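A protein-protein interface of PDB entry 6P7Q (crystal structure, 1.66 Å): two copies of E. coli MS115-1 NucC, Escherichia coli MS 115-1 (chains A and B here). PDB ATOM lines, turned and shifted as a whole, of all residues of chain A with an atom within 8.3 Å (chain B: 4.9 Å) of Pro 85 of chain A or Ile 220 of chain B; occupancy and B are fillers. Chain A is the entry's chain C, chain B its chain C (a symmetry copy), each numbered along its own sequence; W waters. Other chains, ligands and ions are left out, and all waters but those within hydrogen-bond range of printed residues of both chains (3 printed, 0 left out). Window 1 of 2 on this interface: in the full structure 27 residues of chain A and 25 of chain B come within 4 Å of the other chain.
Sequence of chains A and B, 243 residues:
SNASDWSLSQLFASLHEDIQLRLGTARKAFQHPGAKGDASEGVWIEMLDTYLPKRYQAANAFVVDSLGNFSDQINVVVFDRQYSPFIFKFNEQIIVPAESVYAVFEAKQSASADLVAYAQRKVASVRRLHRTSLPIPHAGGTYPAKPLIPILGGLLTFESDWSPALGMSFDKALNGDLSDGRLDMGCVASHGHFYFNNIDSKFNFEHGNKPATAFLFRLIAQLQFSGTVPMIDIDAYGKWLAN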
ATOM      1  N   VAL A  64      -7.352  -5.680 -32.846  1.00  0.00           N
ATOM      2  CA  VAL A  64      -7.968  -6.524 -33.868  1.00  0.00           C
ATOM      3  C   VAL A  64      -8.767  -7.601 -33.141  1.00  0.00           C
ATOM      4  O   VAL A  64      -8.484  -7.914 -31.973  1.00  0.00           O
ATOM      5  CB  VAL A  64      -6.886  -7.125 -34.784  1.00  0.00           C
ATOM      6  CG1 VAL A  64      -6.012  -8.065 -33.965  1.00  0.00           C
ATOM      7  CG2 VAL A  64      -7.463  -7.823 -35.959  1.00  0.00           C
ATOM      8  N   PHE A  79      -3.534  -2.576 -21.711  1.00  0.00           N
ATOM      9  CA  PHE A  79      -3.866  -3.951 -22.102  1.00  0.00           C
ATOM     10  C   PHE A  79      -3.051  -4.965 -21.299  1.00  0.00           C
ATOM     11  O   PHE A  79      -2.095  -4.637 -20.585  1.00  0.00           O
ATOM     12  CB  PHE A  79      -3.651  -4.158 -23.635  1.00  0.00           C
ATOM     13  CG  PHE A  79      -2.223  -3.913 -24.110  1.00  0.00           C
ATOM     14  CD1 PHE A  79      -1.738  -2.632 -24.340  1.00  0.00           C
ATOM     15  CD2 PHE A  79      -1.349  -4.975 -24.361  1.00  0.00           C
ATOM     16  CE1 PHE A  79      -0.458  -2.415 -24.805  1.00  0.00           C
ATOM     17  CE2 PHE A  79      -0.093  -4.779 -24.782  1.00  0.00           C
ATOM     18  CZ  PHE A  79       0.385  -3.469 -25.016  1.00  0.00           C
ATOM     19  N   ASP A  80      -3.552  -6.192 -21.319  1.00  0.00           N
ATOM     20  CA  ASP A  80      -2.870  -7.324 -20.723  1.00  0.00           C
ATOM     21  C   ASP A  80      -1.842  -7.948 -21.665  1.00  0.00           C
ATOM     22  O   ASP A  80      -2.111  -8.144 -22.861  1.00  0.00           O
ATOM     23  CB  ASP A  80      -3.869  -8.429 -20.363  1.00  0.00           C
ATOM     24  CG  ASP A  80      -3.167  -9.685 -19.887  1.00  0.00           C
ATOM     25  OD1 ASP A  80      -2.619  -9.672 -18.719  1.00  0.00           O
ATOM     26  OD2 ASP A  80      -3.168 -10.706 -20.645  1.00  0.00           O
ATOM     27  N   ARG A  81      -0.703  -8.350 -21.093  1.00  0.00           N
ATOM     28  CA  ARG A  81       0.218  -9.290 -21.756  1.00  0.00           C
ATOM     29  C   ARG A  81       0.564 -10.510 -20.899  1.00  0.00           C
ATOM     30  O   ARG A  81       1.228 -11.403 -21.392  1.00  0.00           O
ATOM     31  CB  ARG A  81       1.534  -8.600 -22.150  1.00  0.00           C
ATOM     32  CG  ARG A  81       1.421  -7.875 -23.478  1.00  0.00           C
ATOM     33  CD  ARG A  81       1.588  -8.839 -24.655  1.00  0.00           C
ATOM     34  NE  ARG A  81       2.962  -9.330 -24.673  1.00  0.00           N
ATOM     35  CZ  ARG A  81       3.330 -10.590 -24.792  1.00  0.00           C
ATOM     36  NH1 ARG A  81       2.417 -11.555 -24.905  1.00  0.00           N
ATOM     37  NH2 ARG A  81       4.619 -10.876 -24.833  1.00  0.00           N
ATOM     38  N   GLN A  82       0.092 -10.587 -19.640  1.00  0.00           N
ATOM     39  CA  GLN A  82       0.431 -11.724 -18.805  1.00  0.00           C
ATOM     40  C   GLN A  82      -0.244 -12.976 -19.303  1.00  0.00           C
ATOM     41  O   GLN A  82       0.305 -14.074 -19.161  1.00  0.00           O
ATOM     42  CB  GLN A  82       0.041 -11.445 -17.354  1.00  0.00           C
ATOM     43  CG  GLN A  82       0.624 -12.446 -16.347  1.00  0.00           C
ATOM     44  CD  GLN A  82       2.104 -12.354 -16.174  1.00  0.00           C
ATOM     45  OE1 GLN A  82       2.767 -11.450 -16.705  1.00  0.00           O
ATOM     46  NE2 GLN A  82       2.657 -13.289 -15.414  1.00  0.00           N
ATOM     47  N   TYR A  83      -1.446 -12.814 -19.848  1.00  0.00           N
ATOM     48  CA  TYR A  83      -2.304 -13.915 -20.289  1.00  0.00           C
ATOM     49  C   TYR A  83      -2.659 -13.856 -21.767  1.00  0.00           C
ATOM     50  O   TYR A  83      -3.414 -14.721 -22.263  1.00  0.00           O
ATOM     51  CB  TYR A  83      -3.591 -13.929 -19.470  1.00  0.00           C
ATOM     52  CG  TYR A  83      -3.313 -14.120 -17.971  1.00  0.00           C
ATOM     53  CD1 TYR A  83      -2.990 -15.368 -17.475  1.00  0.00           C
ATOM     54  CD2 TYR A  83      -3.330 -13.060 -17.108  1.00  0.00           C
ATOM     55  CE1 TYR A  83      -2.682 -15.541 -16.096  1.00  0.00           C
ATOM     56  CE2 TYR A  83      -3.068 -13.228 -15.751  1.00  0.00           C
ATOM     57  CZ  TYR A  83      -2.738 -14.460 -15.276  1.00  0.00           C
ATOM     58  OH  TYR A  83      -2.495 -14.611 -13.915  1.00  0.00           O
ATOM     59  N   SER A  84      -2.126 -12.898 -22.500  1.00  0.00           N
ATOM     60  CA  SER A  84      -2.575 -12.557 -23.834  1.00  0.00           C
ATOM     61  C   SER A  84      -1.352 -12.495 -24.741  1.00  0.00           C
ATOM     62  O   SER A  84      -0.347 -11.836 -24.373  1.00  0.00           O
ATOM     63  CB  SER A  84      -3.294 -11.178 -23.898  1.00  0.00           C
ATOM     64  OG  SER A  84      -4.428 -11.130 -22.982  1.00  0.00           O
ATOM     65  N   PRO A  85      -1.389 -13.137 -25.910  1.00  0.00           N
ATOM     66  CA  PRO A  85      -0.359 -12.892 -26.927  1.00  0.00           C
ATOM     67  C   PRO A  85      -0.553 -11.550 -27.609  1.00  0.00           C
ATOM     68  O   PRO A  85      -1.639 -10.974 -27.612  1.00  0.00           O
ATOM     69  CB  PRO A  85      -0.551 -14.040 -27.912  1.00  0.00           C
ATOM     70  CG  PRO A  85      -2.084 -14.261 -27.882  1.00  0.00           C
ATOM     71  CD  PRO A  85      -2.504 -13.942 -26.436  1.00  0.00           C
ATOM     72  N   PHE A  86       0.515 -11.106 -28.275  1.00  0.00           N
ATOM     73  CA  PHE A  86       0.342 -10.189 -29.383  1.00  0.00           C
ATOM     74  C   PHE A  86      -0.237 -10.949 -30.581  1.00  0.00           C
ATOM     75  O   PHE A  86       0.013 -12.133 -30.764  1.00  0.00           O
ATOM     76  CB  PHE A  86       1.685  -9.559 -29.812  1.00  0.00           C
ATOM     77  CG  PHE A  86       2.208  -8.504 -28.874  1.00  0.00           C
ATOM     78  CD1 PHE A  86       1.499  -7.366 -28.639  1.00  0.00           C
ATOM     79  CD2 PHE A  86       3.428  -8.686 -28.251  1.00  0.00           C
ATOM     80  CE1 PHE A  86       1.971  -6.399 -27.731  1.00  0.00           C
ATOM     81  CE2 PHE A  86       3.924  -7.691 -27.381  1.00  0.00           C
ATOM     82  CZ  PHE A  86       3.181  -6.578 -27.124  1.00  0.00           C
ATOM     83  N   ILE A  87      -1.032 -10.265 -31.399  1.00  0.00           N
ATOM     84  CA  ILE A  87      -1.424 -10.824 -32.695  1.00  0.00           C
ATOM     85  C   ILE A  87      -0.322 -10.587 -33.728  1.00  0.00           C
ATOM     86  O   ILE A  87      -0.071 -11.422 -34.581  1.00  0.00           O
ATOM     87  CB  ILE A  87      -2.767 -10.185 -33.133  1.00  0.00           C
ATOM     88  CG1 ILE A  87      -3.928 -10.646 -32.218  1.00  0.00           C
ATOM     89  CG2 ILE A  87      -3.113 -10.496 -34.595  1.00  0.00           C
ATOM     90  CD1 ILE A  87      -4.023 -12.160 -32.087  1.00  0.00           C
ATOM     91  N   PHE A  88       0.351  -9.434 -33.669  1.00  0.00           N
ATOM     92  CA  PHE A  88       1.480  -9.144 -34.560  1.00  0.00           C
ATOM     93  C   PHE A  88       2.367  -8.112 -33.889  1.00  0.00           C
ATOM     94  O   PHE A  88       1.878  -7.122 -33.333  1.00  0.00           O
ATOM     95  CB  PHE A  88       0.978  -8.612 -35.926  1.00  0.00           C
ATOM     96  CG  PHE A  88       2.033  -8.578 -37.011  1.00  0.00           C
ATOM     97  CD1 PHE A  88       2.660  -9.737 -37.399  1.00  0.00           C
ATOM     98  CD2 PHE A  88       2.409  -7.394 -37.595  1.00  0.00           C
ATOM     99  CE1 PHE A  88       3.644  -9.724 -38.358  1.00  0.00           C
ATOM    100  CE2 PHE A  88       3.367  -7.373 -38.549  1.00  0.00           C
ATOM    101  CZ  PHE A  88       3.976  -8.530 -38.966  1.00  0.00           C
ATOM    102  N   ILE A  95       0.097  -4.968 -32.706  1.00  0.00           N
ATOM    103  CA  ILE A  95      -1.339  -5.175 -32.889  1.00  0.00           C
ATOM    104  C   ILE A  95      -1.789  -6.152 -31.825  1.00  0.00           C
ATOM    105  O   ILE A  95      -1.238  -7.248 -31.730  1.00  0.00           O
ATOM    106  CB  ILE A  95      -1.638  -5.703 -34.293  1.00  0.00           C
ATOM    107  CG1 ILE A  95      -1.068  -4.689 -35.317  1.00  0.00           C
ATOM    108  CG2 ILE A  95      -3.165  -5.866 -34.549  1.00  0.00           C
ATOM    109  CD1 ILE A  95      -1.166  -5.101 -36.755  1.00  0.00           C
ATOM    110  N   VAL A  96      -2.734  -5.730 -30.999  1.00  0.00           N
ATOM    111  CA  VAL A  96      -3.152  -6.512 -29.840  1.00  0.00           C
ATOM    112  C   VAL A  96      -4.554  -7.091 -30.048  1.00  0.00           C
ATOM    113  O   VAL A  96      -5.379  -6.500 -30.739  1.00  0.00           O
ATOM    114  CB  VAL A  96      -3.111  -5.670 -28.542  1.00  0.00           C
ATOM    115  CG1 VAL A  96      -1.702  -5.174 -28.263  1.00  0.00           C
ATOM    116  CG2 VAL A  96      -4.091  -4.543 -28.560  1.00  0.00           C
ATOM    117  N   PRO A  97      -4.876  -8.248 -29.476  1.00  0.00           N
ATOM    118  CA  PRO A  97      -6.234  -8.764 -29.628  1.00  0.00           C
ATOM    119  C   PRO A  97      -7.200  -7.991 -28.742  1.00  0.00           C
ATOM    120  O   PRO A  97      -6.848  -7.517 -27.659  1.00  0.00           O
ATOM    121  CB  PRO A  97      -6.109 -10.212 -29.210  1.00  0.00           C
ATOM    122  CG  PRO A  97      -5.018 -10.197 -28.143  1.00  0.00           C
ATOM    123  CD  PRO A  97      -4.015  -9.136 -28.685  1.00  0.00           C
ATOM    124  N   ALA A  98      -8.460  -7.904 -29.192  1.00  0.00           N
ATOM    125  CA  ALA A  98      -9.453  -7.162 -28.420  1.00  0.00           C
ATOM    126  C   ALA A  98      -9.591  -7.681 -27.006  1.00  0.00           C
ATOM    127  O   ALA A  98      -9.848  -6.890 -26.080  1.00  0.00           O
ATOM    128  CB  ALA A  98     -10.803  -7.222 -29.123  1.00  0.00           C
ATOM    129  N   GLU A  99      -9.439  -8.997 -26.825  1.00  0.00           N
ATOM    130  CA  GLU A  99      -9.577  -9.622 -25.509  1.00  0.00           C
ATOM    131  C   GLU A  99      -8.553  -9.100 -24.495  1.00  0.00           C
ATOM    132  O   GLU A  99      -8.765  -9.220 -23.283  1.00  0.00           O
ATOM    133  CB  GLU A  99      -9.405 -11.136 -25.634  1.00  0.00           C
ATOM    134  CG  GLU A  99     -10.544 -11.851 -26.393  1.00  0.00           C
ATOM    135  CD  GLU A  99     -10.356 -11.911 -27.902  1.00  0.00           C
ATOM    136  OE1 GLU A  99      -9.410 -11.272 -28.450  1.00  0.00           O
ATOM    137  OE2 GLU A  99     -11.166 -12.616 -28.564  1.00  0.00           O
ATOM    138  N   SER A 100      -7.443  -8.500 -24.948  1.00  0.00           N
ATOM    139  CA  SER A 100      -6.436  -8.028 -24.039  1.00  0.00           C
ATOM    140  C   SER A 100      -6.715  -6.622 -23.501  1.00  0.00           C
ATOM    141  O   SER A 100      -5.999  -6.154 -22.603  1.00  0.00           O
ATOM    142  CB  SER A 100      -5.073  -8.017 -24.716  1.00  0.00           C
ATOM    143  OG  SER A 100      -5.011  -6.950 -25.636  1.00  0.00           O
ATOM    144  N   MET A 231     -10.301 -14.997 -20.668  1.00  0.00           N
ATOM    145  CA  MET A 231      -9.319 -15.842 -21.321  1.00  0.00           C
ATOM    146  C   MET A 231      -9.619 -15.976 -22.807  1.00  0.00           C
ATOM    147  O   MET A 231     -10.687 -16.476 -23.207  1.00  0.00           O
ATOM    148  CB  MET A 231      -9.232 -17.212 -20.655  1.00  0.00           C
ATOM    149  CG  MET A 231      -8.138 -18.092 -21.278  1.00  0.00           C
ATOM    150  SD  MET A 231      -7.709 -19.575 -20.375  1.00  0.00           S
ATOM    151  CE  MET A 231      -8.792 -20.787 -21.161  1.00  0.00           C
ATOM    152  N   ILE A 232      -8.651 -15.553 -23.622  1.00  0.00           N
ATOM    153  CA  ILE A 232      -8.763 -15.542 -25.070  1.00  0.00           C
ATOM    154  C   ILE A 232      -8.853 -16.949 -25.653  1.00  0.00           C
ATOM    155  O   ILE A 232      -8.191 -17.903 -25.209  1.00  0.00           O
ATOM    156  CB  ILE A 232      -7.582 -14.770 -25.669  1.00  0.00           C
ATOM    157  CG1 ILE A 232      -7.735 -14.564 -27.176  1.00  0.00           C
ATOM    158  CG2 ILE A 232      -6.264 -15.523 -25.362  1.00  0.00           C
ATOM    159  CD1 ILE A 232      -6.632 -13.646 -27.737  1.00  0.00           C
ATOM    160  N   ASP A 233      -9.694 -17.082 -26.681  1.00  0.00           N
ATOM    161  CA  ASP A 233      -9.746 -18.296 -27.506  1.00  0.00           C
ATOM    162  C   ASP A 233      -8.879 -18.070 -28.739  1.00  0.00           C
ATOM    163  O   ASP A 233      -9.333 -17.482 -29.730  1.00  0.00           O
ATOM    164  CB  ASP A 233     -11.184 -18.600 -27.925  1.00  0.00           C
ATOM    165  CG  ASP A 233     -11.295 -19.876 -28.736  1.00  0.00           C
ATOM    166  OD1 ASP A 233     -10.253 -20.488 -29.056  1.00  0.00           O
ATOM    167  OD2 ASP A 233     -12.437 -20.255 -29.050  1.00  0.00           O
ATOM    168  N   ILE A 234      -7.589 -18.445 -28.647  1.00  0.00           N
ATOM    169  CA  ILE A 234      -6.714 -18.161 -29.782  1.00  0.00           C
ATOM    170  C   ILE A 234      -7.120 -18.972 -31.011  1.00  0.00           C
ATOM    171  O   ILE A 234      -6.819 -18.569 -32.145  1.00  0.00           O
ATOM    172  CB  ILE A 234      -5.244 -18.381 -29.391  1.00  0.00           C
ATOM    173  CG1 ILE A 234      -4.325 -17.716 -30.398  1.00  0.00           C
ATOM    174  CG2 ILE A 234      -4.880 -19.863 -29.302  1.00  0.00           C
ATOM    175  CD1 ILE A 234      -4.395 -16.236 -30.396  1.00  0.00           C
ATOM    176  N   ASP A 235      -7.830 -20.084 -30.841  1.00  0.00           N
ATOM    177  CA  ASP A 235      -8.249 -20.857 -32.013  1.00  0.00           C
ATOM    178  C   ASP A 235      -9.338 -20.133 -32.812  1.00  0.00           C
ATOM    179  O   ASP A 235      -9.497 -20.396 -34.003  1.00  0.00           O
ATOM    180  CB  ASP A 235      -8.741 -22.234 -31.591  1.00  0.00           C
ATOM    181  CG  ASP A 235      -7.597 -23.132 -31.120  1.00  0.00           C
ATOM    182  OD1 ASP A 235      -6.477 -23.005 -31.661  1.00  0.00           O
ATOM    183  OD2 ASP A 235      -7.842 -23.936 -30.218  1.00  0.00           O
ATOM    184  N   TYR A 237      -8.958 -16.988 -33.560  1.00  0.00           N
ATOM    185  CA  TYR A 237      -8.080 -16.316 -34.498  1.00  0.00           C
ATOM    186  C   TYR A 237      -7.504 -17.286 -35.527  1.00  0.00           C
ATOM    187  O   TYR A 237      -7.243 -16.892 -36.663  1.00  0.00           O
ATOM    188  CB  TYR A 237      -6.942 -15.601 -33.734  1.00  0.00           C
ATOM    189  CG  TYR A 237      -7.434 -14.373 -32.989  1.00  0.00           C
ATOM    190  CD1 TYR A 237      -7.970 -14.478 -31.701  1.00  0.00           C
ATOM    191  CD2 TYR A 237      -7.408 -13.146 -33.576  1.00  0.00           C
ATOM    192  CE1 TYR A 237      -8.438 -13.353 -31.030  1.00  0.00           C
ATOM    193  CE2 TYR A 237      -7.858 -12.006 -32.938  1.00  0.00           C
ATOM    194  CZ  TYR A 237      -8.363 -12.109 -31.658  1.00  0.00           C
ATOM    195  OH  TYR A 237      -8.826 -11.005 -31.100  1.00  0.00           O
ATOM    196  N   TYR B  51       5.745 -13.627 -28.628  1.00  0.00           N
ATOM    197  CA  TYR B  51       4.306 -13.852 -28.743  1.00  0.00           C
ATOM    198  C   TYR B  51       3.640 -14.559 -27.575  1.00  0.00           C
ATOM    199  O   TYR B  51       2.462 -14.291 -27.312  1.00  0.00           O
ATOM    200  CB  TYR B  51       4.041 -14.640 -30.021  1.00  0.00           C
ATOM    201  CG  TYR B  51       4.160 -13.723 -31.222  1.00  0.00           C
ATOM    202  CD1 TYR B  51       3.169 -12.784 -31.488  1.00  0.00           C
ATOM    203  CD2 TYR B  51       5.279 -13.779 -32.046  1.00  0.00           C
ATOM    204  CE1 TYR B  51       3.287 -11.900 -32.587  1.00  0.00           C
ATOM    205  CE2 TYR B  51       5.393 -12.907 -33.125  1.00  0.00           C
ATOM    206  CZ  TYR B  51       4.395 -12.004 -33.398  1.00  0.00           C
ATOM    207  OH  TYR B  51       4.489 -11.143 -34.486  1.00  0.00           O
ATOM    208  N   LEU B  52       4.332 -15.431 -26.865  1.00  0.00           N
ATOM    209  CA  LEU B  52       3.700 -16.069 -25.714  1.00  0.00           C
ATOM    210  C   LEU B  52       3.288 -15.022 -24.681  1.00  0.00           C
ATOM    211  O   LEU B  52       4.009 -14.044 -24.444  1.00  0.00           O
ATOM    212  CB  LEU B  52       4.636 -17.108 -25.071  1.00  0.00           C
ATOM    213  CG  LEU B  52       4.873 -18.404 -25.850  1.00  0.00           C
ATOM    214  CD1 LEU B  52       5.729 -19.358 -24.991  1.00  0.00           C
ATOM    215  CD2 LEU B  52       3.557 -19.102 -26.246  1.00  0.00           C
ATOM    216  N   PRO B  53       2.161 -15.269 -23.987  1.00  0.00           N
ATOM    217  CA  PRO B  53       1.867 -14.489 -22.783  1.00  0.00           C
ATOM    218  C   PRO B  53       3.070 -14.433 -21.836  1.00  0.00           C
ATOM    219  O   PRO B  53       3.854 -15.362 -21.745  1.00  0.00           O
ATOM    220  CB  PRO B  53       0.696 -15.235 -22.147  1.00  0.00           C
ATOM    221  CG  PRO B  53      -0.009 -15.922 -23.329  1.00  0.00           C
ATOM    222  CD  PRO B  53       1.153 -16.324 -24.267  1.00  0.00           C
ATOM    223  N   LEU B 216       2.301 -22.003 -33.056  1.00  0.00           N
ATOM    224  CA  LEU B 216       2.232 -21.058 -31.945  1.00  0.00           C
ATOM    225  C   LEU B 216       0.857 -21.039 -31.307  1.00  0.00           C
ATOM    226  O   LEU B 216       0.754 -21.049 -30.070  1.00  0.00           O
ATOM    227  CB  LEU B 216       2.616 -19.671 -32.426  1.00  0.00           C
ATOM    228  CG  LEU B 216       2.477 -18.503 -31.476  1.00  0.00           C
ATOM    229  CD1 LEU B 216       3.488 -18.589 -30.312  1.00  0.00           C
ATOM    230  CD2 LEU B 216       2.685 -17.167 -32.248  1.00  0.00           C
ATOM    231  N   PHE B 217      -0.214 -21.019 -32.131  1.00  0.00           N
ATOM    232  CA  PHE B 217      -1.559 -20.975 -31.568  1.00  0.00           C
ATOM    233  C   PHE B 217      -1.910 -22.280 -30.867  1.00  0.00           C
ATOM    234  O   PHE B 217      -2.519 -22.279 -29.791  1.00  0.00           O
ATOM    235  CB  PHE B 217      -2.574 -20.694 -32.669  1.00  0.00           C
ATOM    236  CG  PHE B 217      -2.558 -19.270 -33.184  1.00  0.00           C
ATOM    237  CD1 PHE B 217      -1.618 -18.374 -32.750  1.00  0.00           C
ATOM    238  CD2 PHE B 217      -3.505 -18.860 -34.130  1.00  0.00           C
ATOM    239  CE1 PHE B 217      -1.611 -17.056 -33.191  1.00  0.00           C
ATOM    240  CE2 PHE B 217      -3.484 -17.564 -34.583  1.00  0.00           C
ATOM    241  CZ  PHE B 217      -2.551 -16.668 -34.111  1.00  0.00           C
ATOM    242  N   ARG B 218      -1.504 -23.409 -31.450  1.00  0.00           N
ATOM    243  CA  ARG B 218      -1.704 -24.699 -30.803  1.00  0.00           C
ATOM    244  C   ARG B 218      -1.010 -24.746 -29.435  1.00  0.00           C
ATOM    245  O   ARG B 218      -1.585 -25.270 -28.452  1.00  0.00           O
ATOM    246  CB  ARG B 218      -1.212 -25.801 -31.747  1.00  0.00           C
ATOM    247  CG  ARG B 218      -1.175 -27.199 -31.145  1.00  0.00           C
ATOM    248  CD  ARG B 218      -2.504 -27.815 -31.141  1.00  0.00           C
ATOM    249  NE  ARG B 218      -2.536 -29.055 -30.337  1.00  0.00           N
ATOM    250  CZ  ARG B 218      -3.588 -29.843 -30.217  1.00  0.00           C
ATOM    251  NH1 ARG B 218      -4.698 -29.558 -30.874  1.00  0.00           N
ATOM    252  NH2 ARG B 218      -3.508 -30.928 -29.468  1.00  0.00           N
ATOM    253  N   LEU B 219       0.225 -24.227 -29.357  1.00  0.00           N
ATOM    254  CA  LEU B 219       0.941 -24.196 -28.090  1.00  0.00           C
ATOM    255  C   LEU B 219       0.216 -23.319 -27.076  1.00  0.00           C
ATOM    256  O   LEU B 219       0.038 -23.722 -25.915  1.00  0.00           O
ATOM    257  CB  LEU B 219       2.384 -23.730 -28.311  1.00  0.00           C
ATOM    258  CG  LEU B 219       3.266 -23.627 -27.066  1.00  0.00           C
ATOM    259  CD1 LEU B 219       3.358 -24.933 -26.351  1.00  0.00           C
ATOM    260  CD2 LEU B 219       4.663 -23.124 -27.458  1.00  0.00           C
ATOM    261  N   ILE B 220      -0.214 -22.117 -27.482  1.00  0.00           N
ATOM    262  CA  ILE B 220      -0.901 -21.231 -26.537  1.00  0.00           C
ATOM    263  C   ILE B 220      -2.168 -21.895 -26.007  1.00  0.00           C
ATOM    264  O   ILE B 220      -2.452 -21.882 -24.798  1.00  0.00           O
ATOM    265  CB  ILE B 220      -1.201 -19.866 -27.188  1.00  0.00           C
ATOM    266  CG1 ILE B 220       0.142 -19.131 -27.408  1.00  0.00           C
ATOM    267  CG2 ILE B 220      -2.144 -19.064 -26.313  1.00  0.00           C
ATOM    268  CD1 ILE B 220      -0.037 -17.871 -28.234  1.00  0.00           C
ATOM    269  N   ALA B 221      -2.949 -22.488 -26.908  1.00  0.00           N
ATOM    270  CA  ALA B 221      -4.209 -23.109 -26.511  1.00  0.00           C
ATOM    271  C   ALA B 221      -3.986 -24.286 -25.574  1.00  0.00           C
ATOM    272  O   ALA B 221      -4.729 -24.457 -24.597  1.00  0.00           O
ATOM    273  CB  ALA B 221      -4.971 -23.560 -27.766  1.00  0.00           C
ATOM    274  N   GLN B 222      -2.975 -25.115 -25.858  1.00  0.00           N
ATOM    275  CA  GLN B 222      -2.703 -26.261 -25.002  1.00  0.00           C
ATOM    276  C   GLN B 222      -2.145 -25.807 -23.650  1.00  0.00           C
ATOM    277  O   GLN B 222      -2.538 -26.342 -22.613  1.00  0.00           O
ATOM    278  CB  GLN B 222      -1.727 -27.225 -25.668  1.00  0.00           C
ATOM    279  CG  GLN B 222      -2.310 -27.973 -26.832  1.00  0.00           C
ATOM    280  CD  GLN B 222      -3.581 -28.736 -26.446  1.00  0.00           C
ATOM    281  OE1 GLN B 222      -4.692 -28.418 -26.932  1.00  0.00           O
ATOM    282  NE2 GLN B 222      -3.437 -29.690 -25.543  1.00  0.00           N
ATOM    283  N   LEU B 223      -1.263 -24.792 -23.643  1.00  0.00           N
ATOM    284  CA  LEU B 223      -0.730 -24.317 -22.369  1.00  0.00           C
ATOM    285  C   LEU B 223      -1.831 -23.816 -21.460  1.00  0.00           C
ATOM    286  O   LEU B 223      -1.738 -23.982 -20.238  1.00  0.00           O
ATOM    287  CB  LEU B 223       0.305 -23.200 -22.580  1.00  0.00           C
ATOM    288  CG  LEU B 223       1.664 -23.677 -23.120  1.00  0.00           C
ATOM    289  CD1 LEU B 223       2.507 -22.483 -23.538  1.00  0.00           C
ATOM    290  CD2 LEU B 223       2.338 -24.496 -22.049  1.00  0.00           C
ATOM    291  N   GLN B 224      -2.878 -23.199 -22.023  1.00  0.00           N
ATOM    292  CA  GLN B 224      -3.954 -22.672 -21.183  1.00  0.00           C
ATOM    293  C   GLN B 224      -4.517 -23.732 -20.257  1.00  0.00           C
ATOM    294  O   GLN B 224      -4.889 -23.417 -19.108  1.00  0.00           O
ATOM    295  CB  GLN B 224      -5.091 -22.078 -22.062  1.00  0.00           C
ATOM    296  CG  GLN B 224      -4.745 -20.700 -22.557  1.00  0.00           C
ATOM    297  CD  GLN B 224      -5.783 -20.133 -23.508  1.00  0.00           C
ATOM    298  OE1 GLN B 224      -6.551 -20.869 -24.100  1.00  0.00           O
ATOM    299  NE2 GLN B 224      -5.813 -18.825 -23.632  1.00  0.00           N
HETATM  300  O   HOH W   1       6.474 -13.541 -23.875  1.00  0.00           O
HETATM  301  O   HOH W   2      -7.110 -20.481 -26.754  1.00  0.00           O
HETATM  302  O   HOH W   3      -4.688 -16.944 -21.483  1.00  0.00           O
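The guanidinium group of Arg 81 of chain A lies within hydrogen-bond range of the backbone carbonyl oxygen of Leu 52 of chain B, at 3.0 Å.
The side-chain amide nitrogen (NE2) of Gln 224 of chain B lies within hydrogen-bond range of the backbone carbonyl oxygen (O) of Ile 232 of chain A.
The side-chain carboxylate (OD1) of Asp 80 of chain A lies within hydrogen-bond range of the backbone NH (N) of Gln 82 of chain A (3.0 Å).
The side-chain hydroxyl (OG) of Ser 84 of chain A lies within hydrogen-bond range of the side-chain carboxylate (OD2) of Asp 80 of chain A (2.7 Å).
The guanidinium group (NH1) of Arg 81 of chain A lies within hydrogen-bond range of the backbone carbonyl oxygen (O) of Ser 84 of chain A, 2.8 Å away.
N of Ile 87 of chain A lies within hydrogen-bond range of O of Ile 95 of chain A (3.0 Å).
The backbone carbonyl oxygen (O) of Phe 88 of chain A is in hydrogen-bond range of the backbone NH (N) of Ile 95 of chain A (2.9 Å).
OD1 of Asp 233 of chain A is in hydrogen-bond range of N of Asp 235 of chain A (3.0 Å).
Among the printed residues, merely in contact across the chains: Arg 81 of chain A with Tyr 51 of chain B, Arg 81 of chain A with Pro 53 of chain B, Gln 82 of chain A with Pro 53 of chain B, Tyr 83 of chain A with Pro 53 of chain B, Ser 84 of chain A with Pro 53 of chain B, Pro 85 of chain A with Tyr 51 of chain B, Pro 85 of chain A with Ile 220 of chain B, Phe 86 of chain A with Tyr 51 of chain B, Ile 87 of chain A with Tyr 51 of chain B, Phe 88 of chain A with Tyr 51 of chain B, Met 231 of chain A with Gln 224 of chain B, Ile 234 of chain A with Phe 217 of chain B and Asp 235 of chain A with Ala 221 of chain B.
Of chain B, only Tyr 51 (3.1 Å) and Ile 220 (3.9 Å) come within 4 Å of Pro 85 of chain A.
Ile 220 of chain B touches one residue of chain A.
Of the printed residues of chain B, Tyr 83 of chain A touches Pro 53.
Of the printed residues of chain B, Met 231 of chain A touches Gln 224.
Of the printed residues of chain B, Ile 87 of chain A touches Tyr 51 (3.9 Å).
Of the printed residues of chain B, Ile 232 of chain A touches Gln 224.
Of the printed residues of chain B, Ile 234 of chain A touches Phe 217.
Of the 12 printed residues of chain B, 7 touch a printed residue of chain A.
Hydrophobic or aromatic side chains of chain B that line the printed part of chain A: Tyr 51, Pro 53, Phe 217, Ile 220 and Ala 221.
No position is printed for both chains.
Of the 15 pairs that touch across the chains among the printed residues, none has its exchanged pair printed and touching as well.
Water W1 lies within hydrogen-bond range of the backbone carbonyl oxygen of Leu 52 of chain B (2.6 Å) and the guanidinium group of Arg 81 of chain A (3.4 Å).
Water W3 bridges O of Tyr 83 of chain A and NE2 of Gln 224 of chain B.
Water W2 lies within hydrogen-bond range of OE1 of Gln 224 of chain B (2.7 Å), N of Ile 234 of chain A (2.8 Å) and O of Ile 232 of chain A (3.2 Å).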
